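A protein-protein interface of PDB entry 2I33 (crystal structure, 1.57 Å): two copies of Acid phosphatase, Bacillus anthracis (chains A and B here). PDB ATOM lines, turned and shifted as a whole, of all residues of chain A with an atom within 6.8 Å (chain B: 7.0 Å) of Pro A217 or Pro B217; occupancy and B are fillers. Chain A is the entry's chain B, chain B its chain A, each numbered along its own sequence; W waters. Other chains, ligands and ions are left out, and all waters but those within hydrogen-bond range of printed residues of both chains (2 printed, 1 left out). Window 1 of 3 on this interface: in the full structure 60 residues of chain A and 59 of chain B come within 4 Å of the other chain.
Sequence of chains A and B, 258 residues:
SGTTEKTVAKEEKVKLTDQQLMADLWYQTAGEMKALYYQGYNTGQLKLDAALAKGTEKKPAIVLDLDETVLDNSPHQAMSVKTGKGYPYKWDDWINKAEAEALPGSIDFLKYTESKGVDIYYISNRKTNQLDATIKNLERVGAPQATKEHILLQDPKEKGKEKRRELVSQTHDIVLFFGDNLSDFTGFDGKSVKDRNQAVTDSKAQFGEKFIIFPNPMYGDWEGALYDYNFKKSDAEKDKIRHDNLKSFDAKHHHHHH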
ATOM      1  N   GLN A  20     -21.323 -11.256  29.983  1.00  0.00           N
ATOM      2  CA  GLN A  20     -22.579 -10.628  30.366  1.00  0.00           C
ATOM      3  C   GLN A  20     -22.386  -9.627  31.493  1.00  0.00           C
ATOM      4  O   GLN A  20     -23.343  -8.934  31.867  1.00  0.00           O
ATOM      5  CB  GLN A  20     -23.593 -11.674  30.848  1.00  0.00           C
ATOM      6  CG  GLN A  20     -25.043 -11.201  30.698  1.00  0.00           C
ATOM      7  CD  GLN A  20     -26.072 -12.114  31.357  1.00  0.00           C
ATOM      8  OE1 GLN A  20     -27.153 -12.373  30.764  1.00  0.00           O
ATOM      9  NE2 GLN A  20     -25.765 -12.604  32.559  1.00  0.00           N
ATOM     10  N   MET A  22     -20.930  -6.750  32.350  1.00  0.00           N
ATOM     11  CA  MET A  22     -21.229  -5.300  32.311  1.00  0.00           C
ATOM     12  C   MET A  22     -22.699  -5.027  32.009  1.00  0.00           C
ATOM     13  O   MET A  22     -23.308  -4.127  32.584  1.00  0.00           O
ATOM     14  CB  MET A  22     -20.337  -4.579  31.325  1.00  0.00           C
ATOM     15  CG  MET A  22     -18.931  -4.504  31.814  1.00  0.00           C
ATOM     16  SD  MET A  22     -18.753  -3.398  33.236  1.00  0.00           S
ATOM     17  CE  MET A  22     -18.536  -1.816  32.447  1.00  0.00           C
ATOM     18  N   ALA A  23     -23.260  -5.796  31.099  1.00  0.00           N
ATOM     19  CA  ALA A  23     -24.710  -5.692  30.805  1.00  0.00           C
ATOM     20  C   ALA A  23     -25.551  -5.868  32.093  1.00  0.00           C
ATOM     21  O   ALA A  23     -26.481  -5.112  32.378  1.00  0.00           O
ATOM     22  CB  ALA A  23     -25.103  -6.703  29.772  1.00  0.00           C
ATOM     23  N   ASP A  24     -25.215  -6.887  32.874  1.00  0.00           N
ATOM     24  CA  ASP A  24     -25.924  -7.159  34.125  1.00  0.00           C
ATOM     25  C   ASP A  24     -25.699  -6.049  35.134  1.00  0.00           C
ATOM     26  O   ASP A  24     -26.604  -5.666  35.876  1.00  0.00           O
ATOM     27  CB  ASP A  24     -25.451  -8.466  34.756  1.00  0.00           C
ATOM     28  CG  ASP A  24     -25.851  -9.693  33.960  1.00  0.00           C
ATOM     29  OD1 ASP A  24     -26.632  -9.564  33.014  1.00  0.00           O
ATOM     30  OD2 ASP A  24     -25.371 -10.822  34.318  1.00  0.00           O
ATOM     31  N   TRP A  26     -24.883  -2.966  34.635  1.00  0.00           N
ATOM     32  CA  TRP A  26     -25.646  -1.772  34.230  1.00  0.00           C
ATOM     33  C   TRP A  26     -27.112  -1.952  34.618  1.00  0.00           C
ATOM     34  O   TRP A  26     -27.740  -1.080  35.237  1.00  0.00           O
ATOM     35  CB  TRP A  26     -25.528  -1.550  32.730  1.00  0.00           C
ATOM     36  CG  TRP A  26     -26.285  -0.344  32.233  1.00  0.00           C
ATOM     37  CD1 TRP A  26     -25.859   0.957  32.238  1.00  0.00           C
ATOM     38  CD2 TRP A  26     -27.615  -0.313  31.689  1.00  0.00           C
ATOM     39  NE1 TRP A  26     -26.825   1.777  31.711  1.00  0.00           N
ATOM     40  CE2 TRP A  26     -27.907   1.027  31.357  1.00  0.00           C
ATOM     41  CE3 TRP A  26     -28.564  -1.298  31.384  1.00  0.00           C
ATOM     42  CZ2 TRP A  26     -29.124   1.408  30.769  1.00  0.00           C
ATOM     43  CZ3 TRP A  26     -29.776  -0.916  30.825  1.00  0.00           C
ATOM     44  CH2 TRP A  26     -30.049   0.421  30.515  1.00  0.00           C
ATOM     45  N   TYR A  27     -27.666  -3.102  34.285  1.00  0.00           N
ATOM     46  CA  TYR A  27     -29.082  -3.288  34.526  1.00  0.00           C
ATOM     47  C   TYR A  27     -29.423  -3.247  36.009  1.00  0.00           C
ATOM     48  O   TYR A  27     -30.456  -2.688  36.421  1.00  0.00           O
ATOM     49  CB  TYR A  27     -29.507  -4.588  33.910  1.00  0.00           C
ATOM     50  CG  TYR A  27     -30.997  -4.736  33.830  1.00  0.00           C
ATOM     51  CD1 TYR A  27     -31.698  -4.264  32.728  1.00  0.00           C
ATOM     52  CD2 TYR A  27     -31.709  -5.301  34.872  1.00  0.00           C
ATOM     53  CE1 TYR A  27     -33.075  -4.374  32.644  1.00  0.00           C
ATOM     54  CE2 TYR A  27     -33.093  -5.451  34.795  1.00  0.00           C
ATOM     55  CZ  TYR A  27     -33.784  -4.958  33.673  1.00  0.00           C
ATOM     56  OH  TYR A  27     -35.164  -5.100  33.561  1.00  0.00           O
ATOM     57  N   PHE A 214     -38.269  -1.072  26.652  1.00  0.00           N
ATOM     58  CA  PHE A 214     -37.400  -0.964  27.804  1.00  0.00           C
ATOM     59  C   PHE A 214     -36.088  -1.656  27.509  1.00  0.00           C
ATOM     60  O   PHE A 214     -36.042  -2.593  26.695  1.00  0.00           O
ATOM     61  CB  PHE A 214     -38.030  -1.613  29.038  1.00  0.00           C
ATOM     62  CG  PHE A 214     -39.305  -0.945  29.473  1.00  0.00           C
ATOM     63  CD1 PHE A 214     -39.260   0.219  30.200  1.00  0.00           C
ATOM     64  CD2 PHE A 214     -40.520  -1.445  29.128  1.00  0.00           C
ATOM     65  CE1 PHE A 214     -40.421   0.881  30.569  1.00  0.00           C
ATOM     66  CE2 PHE A 214     -41.705  -0.797  29.535  1.00  0.00           C
ATOM     67  CZ  PHE A 214     -41.630   0.373  30.252  1.00  0.00           C
ATOM     68  N   PRO A 215     -35.016  -1.184  28.142  1.00  0.00           N
ATOM     69  CA  PRO A 215     -33.685  -1.699  27.814  1.00  0.00           C
ATOM     70  C   PRO A 215     -33.296  -2.978  28.524  1.00  0.00           C
ATOM     71  O   PRO A 215     -33.293  -3.022  29.729  1.00  0.00           O
ATOM     72  CB  PRO A 215     -32.756  -0.595  28.295  1.00  0.00           C
ATOM     73  CG  PRO A 215     -33.489  -0.035  29.492  1.00  0.00           C
ATOM     74  CD  PRO A 215     -34.948  -0.069  29.114  1.00  0.00           C
ATOM     75  N   ASN A 216     -32.885  -3.975  27.751  1.00  0.00           N
ATOM     76  CA  ASN A 216     -32.385  -5.213  28.330  1.00  0.00           C
ATOM     77  C   ASN A 216     -31.193  -5.759  27.530  1.00  0.00           C
ATOM     78  O   ASN A 216     -31.368  -6.512  26.574  1.00  0.00           O
ATOM     79  CB  ASN A 216     -33.500  -6.222  28.385  1.00  0.00           C
ATOM     80  CG  ASN A 216     -33.013  -7.577  28.887  1.00  0.00           C
ATOM     81  OD1 ASN A 216     -31.851  -7.696  29.293  1.00  0.00           O
ATOM     82  ND2 ASN A 216     -33.861  -8.594  28.805  1.00  0.00           N
ATOM     83  N   PRO A 217     -29.977  -5.351  27.897  1.00  0.00           N
ATOM     84  CA  PRO A 217     -28.773  -5.815  27.205  1.00  0.00           C
ATOM     85  C   PRO A 217     -28.273  -7.158  27.720  1.00  0.00           C
ATOM     86  O   PRO A 217     -27.224  -7.604  27.303  1.00  0.00           O
ATOM     87  CB  PRO A 217     -27.754  -4.727  27.527  1.00  0.00           C
ATOM     88  CG  PRO A 217     -28.190  -4.221  28.881  1.00  0.00           C
ATOM     89  CD  PRO A 217     -29.667  -4.345  28.933  1.00  0.00           C
ATOM     90  N   MET A 218     -29.004  -7.784  28.642  1.00  0.00           N
ATOM     91  CA  MET A 218     -28.549  -9.020  29.268  1.00  0.00           C
ATOM     92  C   MET A 218     -28.826 -10.239  28.394  1.00  0.00           C
ATOM     93  O   MET A 218     -28.036 -11.188  28.365  1.00  0.00           O
ATOM     94  CB  MET A 218     -29.265  -9.229  30.598  1.00  0.00           C
ATOM     95  CG  MET A 218     -29.048  -8.126  31.598  1.00  0.00           C
ATOM     96  SD  MET A 218     -29.832  -8.481  33.185  1.00  0.00           S
ATOM     97  CE  MET A 218     -31.564  -8.264  32.767  1.00  0.00           C
ATOM     98  N   TYR A 219     -29.983 -10.231  27.738  1.00  0.00           N
ATOM     99  CA  TYR A 219     -30.482 -11.383  27.023  1.00  0.00           C
ATOM    100  C   TYR A 219     -31.663 -10.956  26.185  1.00  0.00           C
ATOM    101  O   TYR A 219     -32.268  -9.895  26.401  1.00  0.00           O
ATOM    102  CB  TYR A 219     -30.888 -12.523  28.004  1.00  0.00           C
ATOM    103  CG  TYR A 219     -32.152 -12.231  28.761  1.00  0.00           C
ATOM    104  CD1 TYR A 219     -33.377 -12.462  28.169  1.00  0.00           C
ATOM    105  CD2 TYR A 219     -32.119 -11.701  30.056  1.00  0.00           C
ATOM    106  CE1 TYR A 219     -34.550 -12.177  28.800  1.00  0.00           C
ATOM    107  CE2 TYR A 219     -33.314 -11.399  30.728  1.00  0.00           C
ATOM    108  CZ  TYR A 219     -34.523 -11.630  30.069  1.00  0.00           C
ATOM    109  OH  TYR A 219     -35.708 -11.350  30.680  1.00  0.00           O
ATOM    110  N   GLY A 220     -32.048 -11.822  25.265  1.00  0.00           N
ATOM    111  CA  GLY A 220     -33.240 -11.538  24.497  1.00  0.00           C
ATOM    112  C   GLY A 220     -33.147 -12.073  23.095  1.00  0.00           C
ATOM    113  O   GLY A 220     -32.178 -12.743  22.716  1.00  0.00           O
ATOM    114  N   TRP A 222     -32.559 -10.313  20.632  1.00  0.00           N
ATOM    115  CA  TRP A 222     -31.423  -9.714  19.951  1.00  0.00           C
ATOM    116  C   TRP A 222     -30.242 -10.675  19.908  1.00  0.00           C
ATOM    117  O   TRP A 222     -29.506 -10.683  18.951  1.00  0.00           O
ATOM    118  CB  TRP A 222     -31.016  -8.397  20.593  1.00  0.00           C
ATOM    119  CG  TRP A 222     -30.511  -8.548  21.959  1.00  0.00           C
ATOM    120  CD1 TRP A 222     -31.218  -8.491  23.102  1.00  0.00           C
ATOM    121  CD2 TRP A 222     -29.142  -8.724  22.338  1.00  0.00           C
ATOM    122  NE1 TRP A 222     -30.402  -8.670  24.168  1.00  0.00           N
ATOM    123  CE2 TRP A 222     -29.116  -8.821  23.736  1.00  0.00           C
ATOM    124  CE3 TRP A 222     -27.944  -8.867  21.625  1.00  0.00           C
ATOM    125  CZ2 TRP A 222     -27.937  -8.979  24.451  1.00  0.00           C
ATOM    126  CZ3 TRP A 222     -26.768  -9.027  22.346  1.00  0.00           C
ATOM    127  CH2 TRP A 222     -26.784  -9.096  23.733  1.00  0.00           C
ATOM    128  N   GLN B  19     -15.658  -8.503  29.528  1.00  0.00           N
ATOM    129  CA  GLN B  19     -16.879  -8.282  30.312  1.00  0.00           C
ATOM    130  C   GLN B  19     -17.869  -7.306  29.681  1.00  0.00           C
ATOM    131  O   GLN B  19     -19.050  -7.252  30.091  1.00  0.00           O
ATOM    132  CB  GLN B  19     -16.494  -7.847  31.727  1.00  0.00           C
ATOM    133  CG  GLN B  19     -15.719  -8.923  32.462  1.00  0.00           C
ATOM    134  CD  GLN B  19     -15.255  -8.479  33.821  1.00  0.00           C
ATOM    135  OE1 GLN B  19     -15.617  -7.401  34.266  1.00  0.00           O
ATOM    136  NE2 GLN B  19     -14.492  -9.324  34.510  1.00  0.00           N
ATOM    137  N   GLN B  20     -17.401  -6.547  28.681  1.00  0.00           N
ATOM    138  CA  GLN B  20     -18.175  -5.541  27.916  1.00  0.00           C
ATOM    139  C   GLN B  20     -18.940  -6.152  26.755  1.00  0.00           C
ATOM    140  O   GLN B  20     -19.778  -5.485  26.119  1.00  0.00           O
ATOM    141  CB  GLN B  20     -17.232  -4.548  27.208  1.00  0.00           C
ATOM    142  CG  GLN B  20     -16.113  -3.932  28.006  1.00  0.00           C
ATOM    143  CD  GLN B  20     -15.247  -2.996  27.157  1.00  0.00           C
ATOM    144  OE1 GLN B  20     -15.479  -2.815  25.941  1.00  0.00           O
ATOM    145  NE2 GLN B  20     -14.242  -2.394  27.789  1.00  0.00           N
ATOM    146  N   MET B  22     -21.241  -8.419  25.767  1.00  0.00           N
ATOM    147  CA  MET B  22     -22.688  -8.440  25.544  1.00  0.00           C
ATOM    148  C   MET B  22     -23.292  -7.038  25.477  1.00  0.00           C
ATOM    149  O   MET B  22     -24.135  -6.745  24.631  1.00  0.00           O
ATOM    150  CB  MET B  22     -23.365  -9.239  26.642  1.00  0.00           C
ATOM    151  CG  MET B  22     -23.140 -10.683  26.475  1.00  0.00           C
ATOM    152  SD  MET B  22     -23.891 -11.312  24.959  1.00  0.00           S
ATOM    153  CE  MET B  22     -25.558 -11.597  25.526  1.00  0.00           C
ATOM    154  N   ALA B  23     -22.862  -6.164  26.375  1.00  0.00           N
ATOM    155  CA  ALA B  23     -23.342  -4.780  26.329  1.00  0.00           C
ATOM    156  C   ALA B  23     -23.058  -4.149  24.959  1.00  0.00           C
ATOM    157  O   ALA B  23     -23.928  -3.487  24.370  1.00  0.00           O
ATOM    158  CB  ALA B  23     -22.705  -3.980  27.395  1.00  0.00           C
ATOM    159  N   ASP B  24     -21.843  -4.363  24.466  1.00  0.00           N
ATOM    160  CA  ASP B  24     -21.416  -3.784  23.185  1.00  0.00           C
ATOM    161  C   ASP B  24     -22.187  -4.393  22.043  1.00  0.00           C
ATOM    162  O   ASP B  24     -22.629  -3.694  21.125  1.00  0.00           O
ATOM    163  CB  ASP B  24     -19.934  -4.059  22.938  1.00  0.00           C
ATOM    164  CG  ASP B  24     -19.023  -3.281  23.840  1.00  0.00           C
ATOM    165  OD1 ASP B  24     -19.493  -2.413  24.608  1.00  0.00           O
ATOM    166  OD2 ASP B  24     -17.801  -3.548  23.780  1.00  0.00           O
ATOM    167  N   TRP B  26     -25.156  -5.835  22.146  1.00  0.00           N
ATOM    168  CA  TRP B  26     -26.520  -5.308  22.194  1.00  0.00           C
ATOM    169  C   TRP B  26     -26.568  -3.926  21.538  1.00  0.00           C
ATOM    170  O   TRP B  26     -27.423  -3.599  20.717  1.00  0.00           O
ATOM    171  CB  TRP B  26     -26.999  -5.160  23.649  1.00  0.00           C
ATOM    172  CG  TRP B  26     -28.391  -4.665  23.776  1.00  0.00           C
ATOM    173  CD1 TRP B  26     -29.550  -5.385  23.641  1.00  0.00           C
ATOM    174  CD2 TRP B  26     -28.792  -3.328  24.070  1.00  0.00           C
ATOM    175  NE1 TRP B  26     -30.640  -4.569  23.831  1.00  0.00           N
ATOM    176  CE2 TRP B  26     -30.196  -3.307  24.114  1.00  0.00           C
ATOM    177  CE3 TRP B  26     -28.096  -2.148  24.299  1.00  0.00           C
ATOM    178  CZ2 TRP B  26     -30.914  -2.172  24.382  1.00  0.00           C
ATOM    179  CZ3 TRP B  26     -28.812  -1.011  24.583  1.00  0.00           C
ATOM    180  CH2 TRP B  26     -30.219  -1.021  24.589  1.00  0.00           C
ATOM    181  N   TYR B  27     -25.657  -3.082  21.957  1.00  0.00           N
ATOM    182  CA  TYR B  27     -25.702  -1.704  21.493  1.00  0.00           C
ATOM    183  C   TYR B  27     -25.505  -1.644  19.973  1.00  0.00           C
ATOM    184  O   TYR B  27     -26.164  -0.856  19.268  1.00  0.00           O
ATOM    185  CB  TYR B  27     -24.608  -0.919  22.177  1.00  0.00           C
ATOM    186  CG  TYR B  27     -24.792   0.555  21.953  1.00  0.00           C
ATOM    187  CD1 TYR B  27     -25.611   1.295  22.780  1.00  0.00           C
ATOM    188  CD2 TYR B  27     -24.163   1.204  20.910  1.00  0.00           C
ATOM    189  CE1 TYR B  27     -25.811   2.680  22.575  1.00  0.00           C
ATOM    190  CE2 TYR B  27     -24.373   2.577  20.694  1.00  0.00           C
ATOM    191  CZ  TYR B  27     -25.202   3.300  21.508  1.00  0.00           C
ATOM    192  OH  TYR B  27     -25.389   4.652  21.312  1.00  0.00           O
ATOM    193  N   MET B  33     -32.236  -1.708  20.836  1.00  0.00           N
ATOM    194  CA  MET B  33     -31.455  -0.498  21.051  1.00  0.00           C
ATOM    195  C   MET B  33     -31.957   0.589  20.103  1.00  0.00           C
ATOM    196  O   MET B  33     -32.235   1.688  20.491  1.00  0.00           O
ATOM    197  CB  MET B  33     -29.981  -0.760  20.808  1.00  0.00           C
ATOM    198  CG  MET B  33     -29.102   0.461  20.830  1.00  0.00           C
ATOM    199  SD  MET B  33     -29.060   1.226  19.205  1.00  0.00           S
ATOM    200  CE  MET B  33     -27.587   2.246  19.335  1.00  0.00           C
ATOM    201  N   ASP B 180     -27.350   9.967  27.375  1.00  0.00           N
ATOM    202  CA  ASP B 180     -27.256   8.559  27.753  1.00  0.00           C
ATOM    203  C   ASP B 180     -26.656   8.376  29.130  1.00  0.00           C
ATOM    204  O   ASP B 180     -26.511   7.254  29.617  1.00  0.00           O
ATOM    205  CB  ASP B 180     -26.376   7.790  26.778  1.00  0.00           C
ATOM    206  CG  ASP B 180     -24.935   8.287  26.795  1.00  0.00           C
ATOM    207  OD1 ASP B 180     -24.721   9.441  26.351  1.00  0.00           O
ATOM    208  OD2 ASP B 180     -24.054   7.509  27.245  1.00  0.00           O
ATOM    209  N   PHE B 214     -31.288   7.877  26.823  1.00  0.00           N
ATOM    210  CA  PHE B 214     -30.940   6.823  25.885  1.00  0.00           C
ATOM    211  C   PHE B 214     -30.105   5.742  26.569  1.00  0.00           C
ATOM    212  O   PHE B 214     -29.366   6.001  27.505  1.00  0.00           O
ATOM    213  CB  PHE B 214     -30.196   7.404  24.706  1.00  0.00           C
ATOM    214  CG  PHE B 214     -31.037   8.368  23.931  1.00  0.00           C
ATOM    215  CD1 PHE B 214     -31.981   7.906  23.062  1.00  0.00           C
ATOM    216  CD2 PHE B 214     -30.914   9.718  24.099  1.00  0.00           C
ATOM    217  CE1 PHE B 214     -32.823   8.762  22.360  1.00  0.00           C
ATOM    218  CE2 PHE B 214     -31.728  10.585  23.390  1.00  0.00           C
ATOM    219  CZ  PHE B 214     -32.691  10.094  22.529  1.00  0.00           C
ATOM    220  N   PRO B 215     -30.227   4.512  26.070  1.00  0.00           N
ATOM    221  CA  PRO B 215     -29.527   3.392  26.742  1.00  0.00           C
ATOM    222  C   PRO B 215     -28.082   3.203  26.341  1.00  0.00           C
ATOM    223  O   PRO B 215     -27.770   2.981  25.176  1.00  0.00           O
ATOM    224  CB  PRO B 215     -30.349   2.187  26.285  1.00  0.00           C
ATOM    225  CG  PRO B 215     -30.745   2.587  24.862  1.00  0.00           C
ATOM    226  CD  PRO B 215     -31.128   4.040  25.000  1.00  0.00           C
ATOM    227  N   ASN B 216     -27.197   3.202  27.322  1.00  0.00           N
ATOM    228  CA  ASN B 216     -25.782   2.948  27.097  1.00  0.00           C
ATOM    229  C   ASN B 216     -25.208   2.059  28.200  1.00  0.00           C
ATOM    230  O   ASN B 216     -24.676   2.524  29.206  1.00  0.00           O
ATOM    231  CB  ASN B 216     -24.998   4.252  27.038  1.00  0.00           C
ATOM    232  CG  ASN B 216     -23.518   4.009  26.826  1.00  0.00           C
ATOM    233  OD1 ASN B 216     -23.107   2.829  26.670  1.00  0.00           O
ATOM    234  ND2 ASN B 216     -22.728   5.074  26.813  1.00  0.00           N
ATOM    235  N   PRO B 217     -25.314   0.752  27.995  1.00  0.00           N
ATOM    236  CA  PRO B 217     -24.739  -0.197  28.945  1.00  0.00           C
ATOM    237  C   PRO B 217     -23.265  -0.467  28.746  1.00  0.00           C
ATOM    238  O   PRO B 217     -22.736  -1.368  29.407  1.00  0.00           O
ATOM    239  CB  PRO B 217     -25.530  -1.476  28.657  1.00  0.00           C
ATOM    240  CG  PRO B 217     -25.786  -1.370  27.213  1.00  0.00           C
ATOM    241  CD  PRO B 217     -26.022   0.065  26.898  1.00  0.00           C
ATOM    242  N   MET B 218     -22.629   0.240  27.811  1.00  0.00           N
ATOM    243  CA  MET B 218     -21.231  -0.034  27.478  1.00  0.00           C
ATOM    244  C   MET B 218     -20.268   0.633  28.449  1.00  0.00           C
ATOM    245  O   MET B 218     -19.193   0.106  28.766  1.00  0.00           O
ATOM    246  CB  MET B 218     -20.920   0.474  26.076  1.00  0.00           C
ATOM    247  CG  MET B 218     -21.750  -0.201  24.961  1.00  0.00           C
ATOM    248  SD  MET B 218     -21.237   0.391  23.370  1.00  0.00           S
ATOM    249  CE  MET B 218     -21.954   2.050  23.423  1.00  0.00           C
ATOM    250  N   TYR B 219     -20.645   1.824  28.860  1.00  0.00           N
ATOM    251  CA  TYR B 219     -19.773   2.684  29.628  1.00  0.00           C
ATOM    252  C   TYR B 219     -20.563   3.888  30.142  1.00  0.00           C
ATOM    253  O   TYR B 219     -21.690   4.146  29.716  1.00  0.00           O
ATOM    254  CB  TYR B 219     -18.591   3.149  28.777  1.00  0.00           C
ATOM    255  CG  TYR B 219     -18.992   4.201  27.782  1.00  0.00           C
ATOM    256  CD1 TYR B 219     -19.270   3.893  26.477  1.00  0.00           C
ATOM    257  CD2 TYR B 219     -19.126   5.530  28.172  1.00  0.00           C
ATOM    258  CE1 TYR B 219     -19.621   4.849  25.569  1.00  0.00           C
ATOM    259  CE2 TYR B 219     -19.530   6.507  27.265  1.00  0.00           C
ATOM    260  CZ  TYR B 219     -19.788   6.168  25.966  1.00  0.00           C
ATOM    261  OH  TYR B 219     -20.178   7.158  25.095  1.00  0.00           O
ATOM    262  N   GLY B 220     -19.927   4.633  31.030  1.00  0.00           N
ATOM    263  CA  GLY B 220     -20.502   5.856  31.524  1.00  0.00           C
ATOM    264  C   GLY B 220     -20.287   6.044  32.994  1.00  0.00           C
ATOM    265  O   GLY B 220     -19.494   5.325  33.644  1.00  0.00           O
ATOM    266  N   TRP B 222     -22.359   5.381  35.295  1.00  0.00           N
ATOM    267  CA  TRP B 222     -22.846   4.256  36.076  1.00  0.00           C
ATOM    268  C   TRP B 222     -21.667   3.363  36.478  1.00  0.00           C
ATOM    269  O   TRP B 222     -21.640   2.824  37.576  1.00  0.00           O
ATOM    270  CB  TRP B 222     -23.887   3.462  35.292  1.00  0.00           C
ATOM    271  CG  TRP B 222     -23.368   2.789  34.104  1.00  0.00           C
ATOM    272  CD1 TRP B 222     -23.339   3.270  32.828  1.00  0.00           C
ATOM    273  CD2 TRP B 222     -22.842   1.471  34.046  1.00  0.00           C
ATOM    274  NE1 TRP B 222     -22.813   2.327  31.981  1.00  0.00           N
ATOM    275  CE2 TRP B 222     -22.500   1.208  32.708  1.00  0.00           C
ATOM    276  CE3 TRP B 222     -22.638   0.479  35.001  1.00  0.00           C
ATOM    277  CZ2 TRP B 222     -21.972  -0.015  32.309  1.00  0.00           C
ATOM    278  CZ3 TRP B 222     -22.101  -0.732  34.598  1.00  0.00           C
ATOM    279  CH2 TRP B 222     -21.756  -0.955  33.281  1.00  0.00           C
HETATM  280  O   HOH W   1     -25.686   4.397  30.750  1.00  0.00           O
HETATM  281  O   HOH W   2     -33.137  -6.136  24.568  1.00  0.00           O
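The backbone NH of Met A22 sits at hydrogen-bond distance from the backbone carbonyl oxygen of Gln B19, at 3.0 Å.
NE1 of Trp B26 lies within hydrogen-bond range of O of Asn A216 (3.4 Å).
O of Asn B216 sits at hydrogen-bond distance from NE1 of Trp A26 (3.4 Å).
OD1 of Asn A216 sits at hydrogen-bond distance from N of Met A218 (2.9 Å).
OD2 of Asp B180 is in hydrogen-bond range of ND2 of Asn B216.
O of Asn A216 sits at hydrogen-bond distance from NE1 of Trp A222 (3.4 Å).
NE1 of Trp B222 lies within hydrogen-bond range of O of Asn B216.
NE1 of Trp A222 lies within hydrogen-bond range of O of Tyr A219, 3.2 Å away.
OE1 of Gln A20 sits close to O of Met A218.
Gln A20 touches Met B22 (CA to CG, 3.9 Å).
CH2 of Trp B222 touches CE of Met A22, at 3.4 Å.
Pro B217 touches Trp A26 (CA to CG, 3.6 Å).
Trp B222 touches Trp A26 (NE1 to CD1, 3.3 Å).
Pro A217 touches Trp B26 (CA to CG, 3.6 Å).
CB of Pro B217 touches CG of Pro A217, 3.8 Å away.
Met B22 touches Met A218 (CE to O, 3.8 Å).
Met B22 touches Trp A222.
Trp A222 touches Trp B26 (NE1 to CD1, 3.4 Å).
Asp A24 touches none of the printed residues of chain B.
Pro A217 touches just these residues of chain B: Trp B26 (3.6 Å) and Pro B217 (3.8 Å).
Printed residues of chain A within 4 Å of Met B22: Gln A20 (3.9 Å), Met A218 (3.8 Å) and Trp A222 (3.3 Å).
Of the printed residues of chain A, Trp B26 touches Asn A216 (3.4 Å), Pro A217 (3.6 Å) and Trp A222 (3.4 Å).
Of chain A, only Trp A26 and Pro A217 come within 4 Å of Pro B217.
The nearest residue of chain A that does not touch Pro B217 is Met A22 (4.2 Å).
Printed residues of chain B that touch a printed residue of chain A: Gln B19, Met B22, Trp B26, Asn B216, Pro B217 and Trp B222.
Hydrophobic or aromatic side chains of chain B within 4 Å of the printed part of chain A: Met B22, Trp B26, Pro B217 and Trp B222.
Hydrophobic or aromatic side chains of chain A within 4 Å of the printed part of chain B: Met A22, Trp A26, Pro A217 and Trp A222.
Among the printed residues, no Asp or Glu carboxylate lies within 4 Å of a Lys or Arg side-chain nitrogen of the other chain.
Gln A20 touches Met B22, but with the chains exchanged Met A22 does not touch Gln B20 (4.04 Å).
Met A22 touches Trp B222, and with the chains exchanged Trp A222 touches Met B22.
Trp A26 touches Asn B216, and with the chains exchanged Asn A216 touches Trp B26.
Pro B217 touches its own counterpart, Pro A217.
Water W1 lies within hydrogen-bond range of O of Asn B216, NE1 of Trp A26 and O of Asp B180.
Water W2 bridges O of Asn A216 (2.7 Å) and NE1 of Trp B26 (3.0 Å).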
